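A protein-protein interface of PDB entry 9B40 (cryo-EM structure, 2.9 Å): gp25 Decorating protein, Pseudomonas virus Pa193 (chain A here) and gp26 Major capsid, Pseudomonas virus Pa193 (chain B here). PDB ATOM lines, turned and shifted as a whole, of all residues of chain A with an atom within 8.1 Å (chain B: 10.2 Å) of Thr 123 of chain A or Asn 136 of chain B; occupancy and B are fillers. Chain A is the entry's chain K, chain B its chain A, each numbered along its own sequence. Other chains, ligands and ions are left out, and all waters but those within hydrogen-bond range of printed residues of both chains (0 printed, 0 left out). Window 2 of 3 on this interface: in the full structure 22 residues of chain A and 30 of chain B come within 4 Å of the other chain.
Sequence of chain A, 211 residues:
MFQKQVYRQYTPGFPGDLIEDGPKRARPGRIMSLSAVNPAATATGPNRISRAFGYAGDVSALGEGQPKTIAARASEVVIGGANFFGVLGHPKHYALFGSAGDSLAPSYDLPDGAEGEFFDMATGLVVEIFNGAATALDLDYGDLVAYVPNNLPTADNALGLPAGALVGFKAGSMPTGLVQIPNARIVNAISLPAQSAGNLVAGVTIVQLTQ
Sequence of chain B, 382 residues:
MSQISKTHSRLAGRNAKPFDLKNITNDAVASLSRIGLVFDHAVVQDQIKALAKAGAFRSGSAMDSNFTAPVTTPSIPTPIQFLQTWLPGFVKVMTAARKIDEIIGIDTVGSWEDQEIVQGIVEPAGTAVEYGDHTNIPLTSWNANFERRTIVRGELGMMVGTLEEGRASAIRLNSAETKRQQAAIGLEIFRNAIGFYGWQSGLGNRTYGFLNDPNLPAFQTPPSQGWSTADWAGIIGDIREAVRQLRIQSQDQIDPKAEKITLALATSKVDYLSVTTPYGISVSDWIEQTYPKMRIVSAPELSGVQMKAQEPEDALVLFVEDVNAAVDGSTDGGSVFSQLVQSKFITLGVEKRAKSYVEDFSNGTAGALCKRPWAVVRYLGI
The side-chain amide oxygen (OD1) of Asn 136 of chain B lies close to the side-chain carboxylate (OE2) of Glu 20 of chain A (3.3 Å).
The backbone NH of Asp 21 of chain A lies within hydrogen-bond range of the backbone carbonyl oxygen of Ile 137 of chain B, at 2.8 Å.
The backbone carbonyl oxygen (O) of Ile 19 of chain A sits at hydrogen-bond distance from the backbone NH (N) of Leu 139 of chain B (2.4 Å).
The backbone carbonyl oxygen (O) of Ile 137 of chain B sits close to the backbone carbonyl oxygen (O) of Ile 19 of chain A, 3.3 Å away.
The backbone NH of Ile 19 of chain A is in hydrogen-bond range of the backbone carbonyl oxygen of Gly 124 of chain A (3.2 Å).
The backbone carbonyl oxygen of Pro 23 of chain A lies within hydrogen-bond range of the side-chain hydroxyl of Thr 123 of chain A (3.5 Å).
Leu 139 of chain B touches Leu 18 of chain A.
Ile 19 of chain A touches Pro 138 of chain B (O to C, 3.1 Å).
O of Ile 137 of chain B touches CA of Glu 20 of chain A (3.2 Å).
CB of Asn 136 of chain B touches O of Asp 21 of chain A, 3.2 Å away.
CG2 of Thr 123 of chain A touches ND2 of Asn 136 of chain B, at 3.4 Å.
Of chain A, only Glu 20 (3.3 Å), Asp 21 (3.2 Å) and Thr 123 (3.4 Å) come within 4 Å of Asn 136 of chain B.
Glu 20 of chain A touches just these residues of chain B: Asn 136 (3.3 Å) and Ile 137 (3.2 Å).
No residue of chain B comes within 4 Å of Gly 22 of chain A.
Pro 23 of chain A touches none of the printed residues of chain B.
Ala 122 of chain A touches none of the printed residues of chain B.
No residue of chain B comes within 4 Å of Gly 124 of chain A.
Printed residues of chain B within 4 Å of Leu 18 of chain A: Leu 139 (3.7 Å).
Printed residues of chain A within 4 Å of Leu 139 of chain B: Leu 18 and Ile 19.
Of the printed residues of chain A, Ile 137 of chain B touches Ile 19 (3.3 Å), Glu 20 (3.2 Å) and Asp 21 (2.8 Å).
Printed residues of chain B within 4 Å of Ile 19 of chain A: Ile 137, Pro 138 and Leu 139.
The nearest printed residue of chain B that does not touch Leu 18 of chain A is Pro 138 of chain B (6.2 Å).
Printed residues of chain A that touch a printed residue of chain B: Leu 18, Ile 19, Glu 20, Asp 21 and Thr 123.
Along chain A the printed residues that touch a printed residue of chain B span positions 18 to 123.
Hydrophobic or aromatic side chains of chain B that line the printed part of chain A: Leu 139.
Among the printed residues, no Asp or Glu carboxylate lies within 4 Å of a Lys or Arg side-chain nitrogen of the other chain.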
ATOM      1  N   LEU A  18      22.220  15.735 -15.681  1.00  0.00           N
ATOM      2  CA  LEU A  18      23.422  15.213 -16.315  1.00  0.00           C
ATOM      3  C   LEU A  18      23.261  13.715 -16.530  1.00  0.00           C
ATOM      4  O   LEU A  18      22.998  12.974 -15.577  1.00  0.00           O
ATOM      5  CB  LEU A  18      24.655  15.486 -15.453  1.00  0.00           C
ATOM      6  CG  LEU A  18      25.682  16.505 -15.943  1.00  0.00           C
ATOM      7  CD1 LEU A  18      25.006  17.788 -16.270  1.00  0.00           C
ATOM      8  CD2 LEU A  18      26.751  16.740 -14.907  1.00  0.00           C
ATOM      9  N   ILE A  19      23.416  13.269 -17.772  1.00  0.00           N
ATOM     10  CA  ILE A  19      23.478  11.837 -18.046  1.00  0.00           C
ATOM     11  C   ILE A  19      24.910  11.331 -18.040  1.00  0.00           C
ATOM     12  O   ILE A  19      25.221  10.343 -17.376  1.00  0.00           O
ATOM     13  CB  ILE A  19      22.772  11.490 -19.372  1.00  0.00           C
ATOM     14  CG1 ILE A  19      21.290  11.833 -19.276  1.00  0.00           C
ATOM     15  CG2 ILE A  19      22.999  10.026 -19.734  1.00  0.00           C
ATOM     16  CD1 ILE A  19      20.383  10.989 -20.151  1.00  0.00           C
ATOM     17  N   GLU A  20      25.812  11.975 -18.765  1.00  0.00           N
ATOM     18  CA  GLU A  20      27.168  11.467 -18.876  1.00  0.00           C
ATOM     19  C   GLU A  20      28.128  12.261 -18.004  1.00  0.00           C
ATOM     20  O   GLU A  20      28.036  13.487 -17.908  1.00  0.00           O
ATOM     21  CB  GLU A  20      27.631  11.466 -20.330  1.00  0.00           C
ATOM     22  CG  GLU A  20      26.506  11.229 -21.309  1.00  0.00           C
ATOM     23  CD  GLU A  20      26.982  10.557 -22.574  1.00  0.00           C
ATOM     24  OE1 GLU A  20      27.688  11.214 -23.360  1.00  0.00           O
ATOM     25  OE2 GLU A  20      26.653   9.371 -22.781  1.00  0.00           O
ATOM     26  N   ASP A  21      29.043  11.540 -17.364  1.00  0.00           N
ATOM     27  CA  ASP A  21      30.043  12.115 -16.477  1.00  0.00           C
ATOM     28  C   ASP A  21      31.341  12.311 -17.241  1.00  0.00           C
ATOM     29  O   ASP A  21      31.805  11.401 -17.934  1.00  0.00           O
ATOM     30  CB  ASP A  21      30.281  11.212 -15.267  1.00  0.00           C
ATOM     31  CG  ASP A  21      31.171  11.856 -14.227  1.00  0.00           C
ATOM     32  OD1 ASP A  21      30.739  12.847 -13.606  1.00  0.00           O
ATOM     33  OD2 ASP A  21      32.306  11.374 -14.037  1.00  0.00           O
ATOM     34  N   GLY A  22      31.931  13.491 -17.100  1.00  0.00           N
ATOM     35  CA  GLY A  22      33.138  13.831 -17.810  1.00  0.00           C
ATOM     36  C   GLY A  22      33.562  15.248 -17.501  1.00  0.00           C
ATOM     37  O   GLY A  22      33.215  15.806 -16.455  1.00  0.00           O
ATOM     38  N   PRO A  23      34.340  15.856 -18.396  1.00  0.00           N
ATOM     39  CA  PRO A  23      34.734  17.257 -18.197  1.00  0.00           C
ATOM     40  C   PRO A  23      33.520  18.171 -18.260  1.00  0.00           C
ATOM     41  O   PRO A  23      32.800  18.212 -19.260  1.00  0.00           O
ATOM     42  CB  PRO A  23      35.711  17.518 -19.348  1.00  0.00           C
ATOM     43  CG  PRO A  23      35.404  16.479 -20.361  1.00  0.00           C
ATOM     44  CD  PRO A  23      34.941  15.276 -19.607  1.00  0.00           C
ATOM     45  N   LYS A  24      33.290  18.905 -17.174  1.00  0.00           N
ATOM     46  CA  LYS A  24      32.149  19.801 -17.082  1.00  0.00           C
ATOM     47  C   LYS A  24      32.572  21.107 -16.430  1.00  0.00           C
ATOM     48  O   LYS A  24      33.498  21.150 -15.618  1.00  0.00           O
ATOM     49  CB  LYS A  24      30.999  19.186 -16.279  1.00  0.00           C
ATOM     50  CG  LYS A  24      31.365  18.884 -14.845  1.00  0.00           C
ATOM     51  CD  LYS A  24      30.206  18.313 -14.063  1.00  0.00           C
ATOM     52  CE  LYS A  24      30.623  18.091 -12.622  1.00  0.00           C
ATOM     53  NZ  LYS A  24      29.499  17.648 -11.766  1.00  0.00           N
ATOM     54  N   ARG A  25      31.879  22.176 -16.810  1.00  0.00           N
ATOM     55  CA  ARG A  25      32.082  23.515 -16.272  1.00  0.00           C
ATOM     56  C   ARG A  25      30.722  24.132 -15.994  1.00  0.00           C
ATOM     57  O   ARG A  25      29.875  24.195 -16.889  1.00  0.00           O
ATOM     58  CB  ARG A  25      32.884  24.391 -17.248  1.00  0.00           C
ATOM     59  CG  ARG A  25      34.145  23.732 -17.782  1.00  0.00           C
ATOM     60  CD  ARG A  25      35.312  24.663 -17.776  1.00  0.00           C
ATOM     61  NE  ARG A  25      36.276  24.330 -18.817  1.00  0.00           N
ATOM     62  CZ  ARG A  25      36.259  24.813 -20.050  1.00  0.00           C
ATOM     63  NH1 ARG A  25      35.237  25.519 -20.501  1.00  0.00           N
ATOM     64  NH2 ARG A  25      37.276  24.549 -20.862  1.00  0.00           N
ATOM     65  N   PHE A 119      25.226  25.358 -16.170  1.00  0.00           N
ATOM     66  CA  PHE A 119      26.273  24.601 -16.837  1.00  0.00           C
ATOM     67  C   PHE A 119      26.745  25.357 -18.070  1.00  0.00           C
ATOM     68  O   PHE A 119      25.956  25.627 -18.981  1.00  0.00           O
ATOM     69  CB  PHE A 119      25.759  23.217 -17.219  1.00  0.00           C
ATOM     70  CG  PHE A 119      25.618  22.286 -16.055  1.00  0.00           C
ATOM     71  CD1 PHE A 119      26.672  21.481 -15.661  1.00  0.00           C
ATOM     72  CD2 PHE A 119      24.430  22.219 -15.354  1.00  0.00           C
ATOM     73  CE1 PHE A 119      26.540  20.626 -14.588  1.00  0.00           C
ATOM     74  CE2 PHE A 119      24.292  21.368 -14.281  1.00  0.00           C
ATOM     75  CZ  PHE A 119      25.348  20.570 -13.899  1.00  0.00           C
ATOM     76  N   MET A 121      29.409  24.055 -19.754  1.00  0.00           N
ATOM     77  CA  MET A 121      29.689  22.925 -20.626  1.00  0.00           C
ATOM     78  C   MET A 121      29.503  21.631 -19.845  1.00  0.00           C
ATOM     79  O   MET A 121      29.688  21.593 -18.626  1.00  0.00           O
ATOM     80  CB  MET A 121      31.097  23.018 -21.220  1.00  0.00           C
ATOM     81  CG  MET A 121      32.210  22.479 -20.371  1.00  0.00           C
ATOM     82  SD  MET A 121      33.724  22.241 -21.324  1.00  0.00           S
ATOM     83  CE  MET A 121      34.383  20.751 -20.594  1.00  0.00           C
ATOM     84  N   ALA A 122      29.121  20.575 -20.561  1.00  0.00           N
ATOM     85  CA  ALA A 122      28.857  19.283 -19.947  1.00  0.00           C
ATOM     86  C   ALA A 122      28.970  18.197 -21.007  1.00  0.00           C
ATOM     87  O   ALA A 122      28.658  18.433 -22.175  1.00  0.00           O
ATOM     88  CB  ALA A 122      27.469  19.242 -19.299  1.00  0.00           C
ATOM     89  N   THR A 123      29.431  17.014 -20.589  1.00  0.00           N
ATOM     90  CA  THR A 123      29.510  15.883 -21.507  1.00  0.00           C
ATOM     91  C   THR A 123      28.124  15.444 -21.962  1.00  0.00           C
ATOM     92  O   THR A 123      27.913  15.152 -23.145  1.00  0.00           O
ATOM     93  CB  THR A 123      30.253  14.721 -20.849  1.00  0.00           C
ATOM     94  OG1 THR A 123      31.541  15.167 -20.407  1.00  0.00           O
ATOM     95  CG2 THR A 123      30.441  13.584 -21.830  1.00  0.00           C
ATOM     96  N   GLY A 124      27.167  15.394 -21.042  1.00  0.00           N
ATOM     97  CA  GLY A 124      25.793  15.106 -21.401  1.00  0.00           C
ATOM     98  C   GLY A 124      24.798  15.829 -20.519  1.00  0.00           C
ATOM     99  O   GLY A 124      24.824  15.678 -19.295  1.00  0.00           O
ATOM    100  N   LEU A 125      23.913  16.613 -21.128  1.00  0.00           N
ATOM    101  CA  LEU A 125      22.908  17.384 -20.408  1.00  0.00           C
ATOM    102  C   LEU A 125      21.553  17.162 -21.060  1.00  0.00           C
ATOM    103  O   LEU A 125      21.427  17.286 -22.280  1.00  0.00           O
ATOM    104  CB  LEU A 125      23.268  18.878 -20.396  1.00  0.00           C
ATOM    105  CG  LEU A 125      22.435  19.876 -19.586  1.00  0.00           C
ATOM    106  CD1 LEU A 125      22.712  19.772 -18.119  1.00  0.00           C
ATOM    107  CD2 LEU A 125      22.742  21.288 -20.047  1.00  0.00           C
ATOM    108  N   VAL A 126      20.551  16.818 -20.259  1.00  0.00           N
ATOM    109  CA  VAL A 126      19.195  16.701 -20.781  1.00  0.00           C
ATOM    110  C   VAL A 126      18.603  18.099 -20.858  1.00  0.00           C
ATOM    111  O   VAL A 126      18.508  18.802 -19.848  1.00  0.00           O
ATOM    112  CB  VAL A 126      18.327  15.784 -19.910  1.00  0.00           C
ATOM    113  CG1 VAL A 126      17.026  15.475 -20.620  1.00  0.00           C
ATOM    114  CG2 VAL A 126      19.051  14.519 -19.599  1.00  0.00           C
ATOM    115  N   TYR A 141      22.971  13.015 -34.595  1.00  0.00           N
ATOM    116  CA  TYR A 141      24.209  13.207 -33.846  1.00  0.00           C
ATOM    117  C   TYR A 141      24.901  14.511 -34.228  1.00  0.00           C
ATOM    118  O   TYR A 141      25.432  15.219 -33.366  1.00  0.00           O
ATOM    119  CB  TYR A 141      25.142  12.020 -34.082  1.00  0.00           C
ATOM    120  CG  TYR A 141      26.180  11.819 -33.006  1.00  0.00           C
ATOM    121  CD1 TYR A 141      25.823  11.353 -31.753  1.00  0.00           C
ATOM    122  CD2 TYR A 141      27.517  12.098 -33.245  1.00  0.00           C
ATOM    123  CE1 TYR A 141      26.761  11.169 -30.765  1.00  0.00           C
ATOM    124  CE2 TYR A 141      28.467  11.915 -32.261  1.00  0.00           C
ATOM    125  CZ  TYR A 141      28.083  11.450 -31.022  1.00  0.00           C
ATOM    126  OH  TYR A 141      29.022  11.265 -30.035  1.00  0.00           O
ATOM    127  N   ARG A 185      26.229  20.415 -29.371  1.00  0.00           N
ATOM    128  CA  ARG A 185      25.856  19.327 -30.263  1.00  0.00           C
ATOM    129  C   ARG A 185      24.706  18.520 -29.681  1.00  0.00           C
ATOM    130  O   ARG A 185      24.643  18.291 -28.471  1.00  0.00           O
ATOM    131  CB  ARG A 185      27.053  18.412 -30.531  1.00  0.00           C
ATOM    132  CG  ARG A 185      27.608  18.543 -31.934  1.00  0.00           C
ATOM    133  CD  ARG A 185      29.067  18.134 -32.008  1.00  0.00           C
ATOM    134  NE  ARG A 185      29.251  16.690 -32.095  1.00  0.00           N
ATOM    135  CZ  ARG A 185      29.785  15.950 -31.135  1.00  0.00           C
ATOM    136  NH1 ARG A 185      30.204  16.486 -30.001  1.00  0.00           N
ATOM    137  NH2 ARG A 185      29.914  14.640 -31.320  1.00  0.00           N
ATOM    138  N   VAL A 187      23.410  15.122 -29.106  1.00  0.00           N
ATOM    139  CA  VAL A 187      24.005  13.788 -29.076  1.00  0.00           C
ATOM    140  C   VAL A 187      22.980  12.733 -29.473  1.00  0.00           C
ATOM    141  O   VAL A 187      23.138  12.036 -30.480  1.00  0.00           O
ATOM    142  CB  VAL A 187      24.612  13.502 -27.692  1.00  0.00           C
ATOM    143  CG1 VAL A 187      24.910  12.020 -27.530  1.00  0.00           C
ATOM    144  CG2 VAL A 187      25.872  14.317 -27.497  1.00  0.00           C
ATOM    145  N   VAL A 207      19.587  14.584 -25.003  1.00  0.00           N
ATOM    146  CA  VAL A 207      20.955  14.656 -24.506  1.00  0.00           C
ATOM    147  C   VAL A 207      21.750  15.564 -25.431  1.00  0.00           C
ATOM    148  O   VAL A 207      21.713  15.410 -26.657  1.00  0.00           O
ATOM    149  CB  VAL A 207      21.584  13.257 -24.424  1.00  0.00           C
ATOM    150  CG1 VAL A 207      22.986  13.345 -23.849  1.00  0.00           C
ATOM    151  CG2 VAL A 207      20.729  12.337 -23.581  1.00  0.00           C
ATOM    152  N   GLN A 208      22.460  16.522 -24.851  1.00  0.00           N
ATOM    153  CA  GLN A 208      23.267  17.453 -25.616  1.00  0.00           C
ATOM    154  C   GLN A 208      24.657  17.542 -25.003  1.00  0.00           C
ATOM    155  O   GLN A 208      24.838  17.360 -23.794  1.00  0.00           O
ATOM    156  CB  GLN A 208      22.604  18.842 -25.684  1.00  0.00           C
ATOM    157  CG  GLN A 208      23.121  19.853 -24.680  1.00  0.00           C
ATOM    158  CD  GLN A 208      22.814  21.278 -25.079  1.00  0.00           C
ATOM    159  OE1 GLN A 208      22.107  21.519 -26.055  1.00  0.00           O
ATOM    160  NE2 GLN A 208      23.343  22.232 -24.324  1.00  0.00           N
ATOM    161  N   LEU A 209      25.641  17.780 -25.862  1.00  0.00           N
ATOM    162  CA  LEU A 209      27.023  17.983 -25.454  1.00  0.00           C
ATOM    163  C   LEU A 209      27.377  19.433 -25.739  1.00  0.00           C
ATOM    164  O   LEU A 209      27.239  19.895 -26.877  1.00  0.00           O
ATOM    165  CB  LEU A 209      27.964  17.027 -26.188  1.00  0.00           C
ATOM    166  CG  LEU A 209      29.474  17.126 -25.949  1.00  0.00           C
ATOM    167  CD1 LEU A 209      30.074  15.744 -25.956  1.00  0.00           C
ATOM    168  CD2 LEU A 209      30.174  17.979 -26.997  1.00  0.00           C
ATOM    169  N   THR A 210      27.822  20.145 -24.713  1.00  0.00           N
ATOM    170  CA  THR A 210      28.160  21.555 -24.825  1.00  0.00           C
ATOM    171  C   THR A 210      29.661  21.709 -24.633  1.00  0.00           C
ATOM    172  O   THR A 210      30.211  21.223 -23.641  1.00  0.00           O
ATOM    173  CB  THR A 210      27.390  22.381 -23.794  1.00  0.00           C
ATOM    174  OG1 THR A 210      25.991  22.342 -24.102  1.00  0.00           O
ATOM    175  CG2 THR A 210      27.835  23.821 -23.847  1.00  0.00           C
ATOM    176  N   GLN A 211      30.313  22.368 -25.591  1.00  0.00           N
ATOM    177  CA  GLN A 211      31.767  22.546 -25.626  1.00  0.00           C
ATOM    178  C   GLN A 211      32.536  21.240 -25.449  1.00  0.00           C
ATOM    179  O   GLN A 211      32.360  20.298 -26.217  1.00  0.00           O
ATOM    180  CB  GLN A 211      32.216  23.550 -24.567  1.00  0.00           C
ATOM    181  CG  GLN A 211      32.691  24.871 -25.132  1.00  0.00           C
ATOM    182  CD  GLN A 211      32.560  26.007 -24.144  1.00  0.00           C
ATOM    183  OE1 GLN A 211      32.842  25.847 -22.958  1.00  0.00           O
ATOM    184  NE2 GLN A 211      32.130  27.165 -24.628  1.00  0.00           N
ATOM    185  N   THR B 127      19.282   4.972 -18.407  1.00  0.00           N
ATOM    186  CA  THR B 127      19.453   3.923 -19.398  1.00  0.00           C
ATOM    187  C   THR B 127      20.913   3.511 -19.422  1.00  0.00           C
ATOM    188  O   THR B 127      21.806   4.361 -19.357  1.00  0.00           O
ATOM    189  CB  THR B 127      19.022   4.380 -20.796  1.00  0.00           C
ATOM    190  OG1 THR B 127      19.584   5.669 -21.070  1.00  0.00           O
ATOM    191  CG2 THR B 127      17.509   4.462 -20.890  1.00  0.00           C
ATOM    192  N   ALA B 128      21.153   2.208 -19.508  1.00  0.00           N
ATOM    193  CA  ALA B 128      22.516   1.712 -19.535  1.00  0.00           C
ATOM    194  C   ALA B 128      23.178   2.037 -20.869  1.00  0.00           C
ATOM    195  O   ALA B 128      22.534   2.468 -21.826  1.00  0.00           O
ATOM    196  CB  ALA B 128      22.545   0.204 -19.291  1.00  0.00           C
ATOM    197  N   VAL B 129      24.501   1.880 -20.902  1.00  0.00           N
ATOM    198  CA  VAL B 129      25.274   1.913 -22.135  1.00  0.00           C
ATOM    199  C   VAL B 129      26.241   0.740 -22.099  1.00  0.00           C
ATOM    200  O   VAL B 129      26.455   0.115 -21.060  1.00  0.00           O
ATOM    201  CB  VAL B 129      26.053   3.235 -22.352  1.00  0.00           C
ATOM    202  CG1 VAL B 129      25.159   4.450 -22.157  1.00  0.00           C
ATOM    203  CG2 VAL B 129      27.249   3.307 -21.424  1.00  0.00           C
ATOM    204  N   GLU B 130      26.808   0.428 -23.262  1.00  0.00           N
ATOM    205  CA  GLU B 130      27.863  -0.572 -23.322  1.00  0.00           C
ATOM    206  C   GLU B 130      29.074  -0.092 -22.532  1.00  0.00           C
ATOM    207  O   GLU B 130      29.396   1.098 -22.522  1.00  0.00           O
ATOM    208  CB  GLU B 130      28.248  -0.849 -24.772  1.00  0.00           C
ATOM    209  CG  GLU B 130      27.338  -1.833 -25.476  1.00  0.00           C
ATOM    210  CD  GLU B 130      27.170  -1.506 -26.942  1.00  0.00           C
ATOM    211  OE1 GLU B 130      27.037  -0.309 -27.270  1.00  0.00           O
ATOM    212  OE2 GLU B 130      27.173  -2.442 -27.767  1.00  0.00           O
ATOM    213  N   TYR B 131      29.732  -1.019 -21.845  1.00  0.00           N
ATOM    214  CA  TYR B 131      30.859  -0.647 -21.003  1.00  0.00           C
ATOM    215  C   TYR B 131      32.068  -0.250 -21.839  1.00  0.00           C
ATOM    216  O   TYR B 131      32.335  -0.826 -22.897  1.00  0.00           O
ATOM    217  CB  TYR B 131      31.229  -1.792 -20.061  1.00  0.00           C
ATOM    218  CG  TYR B 131      32.540  -1.568 -19.340  1.00  0.00           C
ATOM    219  CD1 TYR B 131      32.614  -0.717 -18.250  1.00  0.00           C
ATOM    220  CD2 TYR B 131      33.703  -2.204 -19.755  1.00  0.00           C
ATOM    221  CE1 TYR B 131      33.808  -0.501 -17.597  1.00  0.00           C
ATOM    222  CE2 TYR B 131      34.899  -1.993 -19.105  1.00  0.00           C
ATOM    223  CZ  TYR B 131      34.944  -1.144 -18.025  1.00  0.00           C
ATOM    224  OH  TYR B 131      36.131  -0.929 -17.369  1.00  0.00           O
ATOM    225  N   GLY B 132      32.804   0.743 -21.347  1.00  0.00           N
ATOM    226  CA  GLY B 132      34.093   1.105 -21.892  1.00  0.00           C
ATOM    227  C   GLY B 132      34.987   1.668 -20.808  1.00  0.00           C
ATOM    228  O   GLY B 132      34.500   2.343 -19.897  1.00  0.00           O
ATOM    229  N   ASP B 133      36.289   1.378 -20.874  1.00  0.00           N
ATOM    230  CA  ASP B 133      37.208   1.878 -19.855  1.00  0.00           C
ATOM    231  C   ASP B 133      37.298   3.396 -19.887  1.00  0.00           C
ATOM    232  O   ASP B 133      37.297   4.050 -18.837  1.00  0.00           O
ATOM    233  CB  ASP B 133      38.593   1.261 -20.043  1.00  0.00           C
ATOM    234  CG  ASP B 133      38.626  -0.210 -19.696  1.00  0.00           C
ATOM    235  OD1 ASP B 133      37.902  -0.617 -18.767  1.00  0.00           O
ATOM    236  OD2 ASP B 133      39.379  -0.959 -20.351  1.00  0.00           O
ATOM    237  N   HIS B 134      37.369   3.975 -21.082  1.00  0.00           N
ATOM    238  CA  HIS B 134      37.536   5.410 -21.248  1.00  0.00           C
ATOM    239  C   HIS B 134      36.256   6.117 -21.664  1.00  0.00           C
ATOM    240  O   HIS B 134      36.275   7.336 -21.862  1.00  0.00           O
ATOM    241  CB  HIS B 134      38.641   5.684 -22.269  1.00  0.00           C
ATOM    242  CG  HIS B 134      39.985   5.186 -21.844  1.00  0.00           C
ATOM    243  ND1 HIS B 134      40.305   4.946 -20.526  1.00  0.00           N
ATOM    244  CD2 HIS B 134      41.092   4.882 -22.561  1.00  0.00           C
ATOM    245  CE1 HIS B 134      41.550   4.513 -20.449  1.00  0.00           C
ATOM    246  NE2 HIS B 134      42.051   4.466 -21.670  1.00  0.00           N
ATOM    247  N   THR B 135      35.149   5.394 -21.797  1.00  0.00           N
ATOM    248  CA  THR B 135      33.883   6.010 -22.157  1.00  0.00           C
ATOM    249  C   THR B 135      33.296   6.750 -20.965  1.00  0.00           C
ATOM    250  O   THR B 135      33.504   6.364 -19.812  1.00  0.00           O
ATOM    251  CB  THR B 135      32.892   4.961 -22.657  1.00  0.00           C
ATOM    252  OG1 THR B 135      32.603   4.035 -21.604  1.00  0.00           O
ATOM    253  CG2 THR B 135      33.472   4.211 -23.842  1.00  0.00           C
ATOM    254  N   ASN B 136      32.578   7.832 -21.254  1.00  0.00           N
ATOM    255  CA  ASN B 136      31.948   8.622 -20.206  1.00  0.00           C
ATOM    256  C   ASN B 136      30.848   7.830 -19.505  1.00  0.00           C
ATOM    257  O   ASN B 136      30.114   7.060 -20.129  1.00  0.00           O
ATOM    258  CB  ASN B 136      31.404   9.923 -20.799  1.00  0.00           C
ATOM    259  CG  ASN B 136      30.693   9.717 -22.123  1.00  0.00           C
ATOM    260  OD1 ASN B 136      29.856   8.829 -22.268  1.00  0.00           O
ATOM    261  ND2 ASN B 136      31.038  10.538 -23.107  1.00  0.00           N
ATOM    262  N   ILE B 137      30.748   8.018 -18.193  1.00  0.00           N
ATOM    263  CA  ILE B 137      29.854   7.226 -17.352  1.00  0.00           C
ATOM    264  C   ILE B 137      28.424   7.745 -17.448  1.00  0.00           C
ATOM    265  O   ILE B 137      28.171   8.916 -17.135  1.00  0.00           O
ATOM    266  CB  ILE B 137      30.326   7.231 -15.889  1.00  0.00           C
ATOM    267  CG1 ILE B 137      31.815   6.894 -15.807  1.00  0.00           C
ATOM    268  CG2 ILE B 137      29.497   6.267 -15.061  1.00  0.00           C
ATOM    269  CD1 ILE B 137      32.418   7.137 -14.447  1.00  0.00           C
ATOM    270  N   PRO B 138      27.466   6.920 -17.864  1.00  0.00           N
ATOM    271  CA  PRO B 138      26.062   7.326 -17.792  1.00  0.00           C
ATOM    272  C   PRO B 138      25.613   7.439 -16.345  1.00  0.00           C
ATOM    273  O   PRO B 138      26.106   6.730 -15.469  1.00  0.00           O
ATOM    274  CB  PRO B 138      25.328   6.195 -18.516  1.00  0.00           C
ATOM    275  CG  PRO B 138      26.207   5.017 -18.313  1.00  0.00           C
ATOM    276  CD  PRO B 138      27.613   5.542 -18.359  1.00  0.00           C
ATOM    277  N   LEU B 139      24.670   8.345 -16.093  1.00  0.00           N
ATOM    278  CA  LEU B 139      24.226   8.613 -14.732  1.00  0.00           C
ATOM    279  C   LEU B 139      22.713   8.500 -14.637  1.00  0.00           C
ATOM    280  O   LEU B 139      21.987   8.966 -15.520  1.00  0.00           O
ATOM    281  CB  LEU B 139      24.671  10.002 -14.251  1.00  0.00           C
ATOM    282  CG  LEU B 139      26.168  10.326 -14.319  1.00  0.00           C
ATOM    283  CD1 LEU B 139      26.402  11.817 -14.144  1.00  0.00           C
ATOM    284  CD2 LEU B 139      26.974   9.524 -13.321  1.00  0.00           C
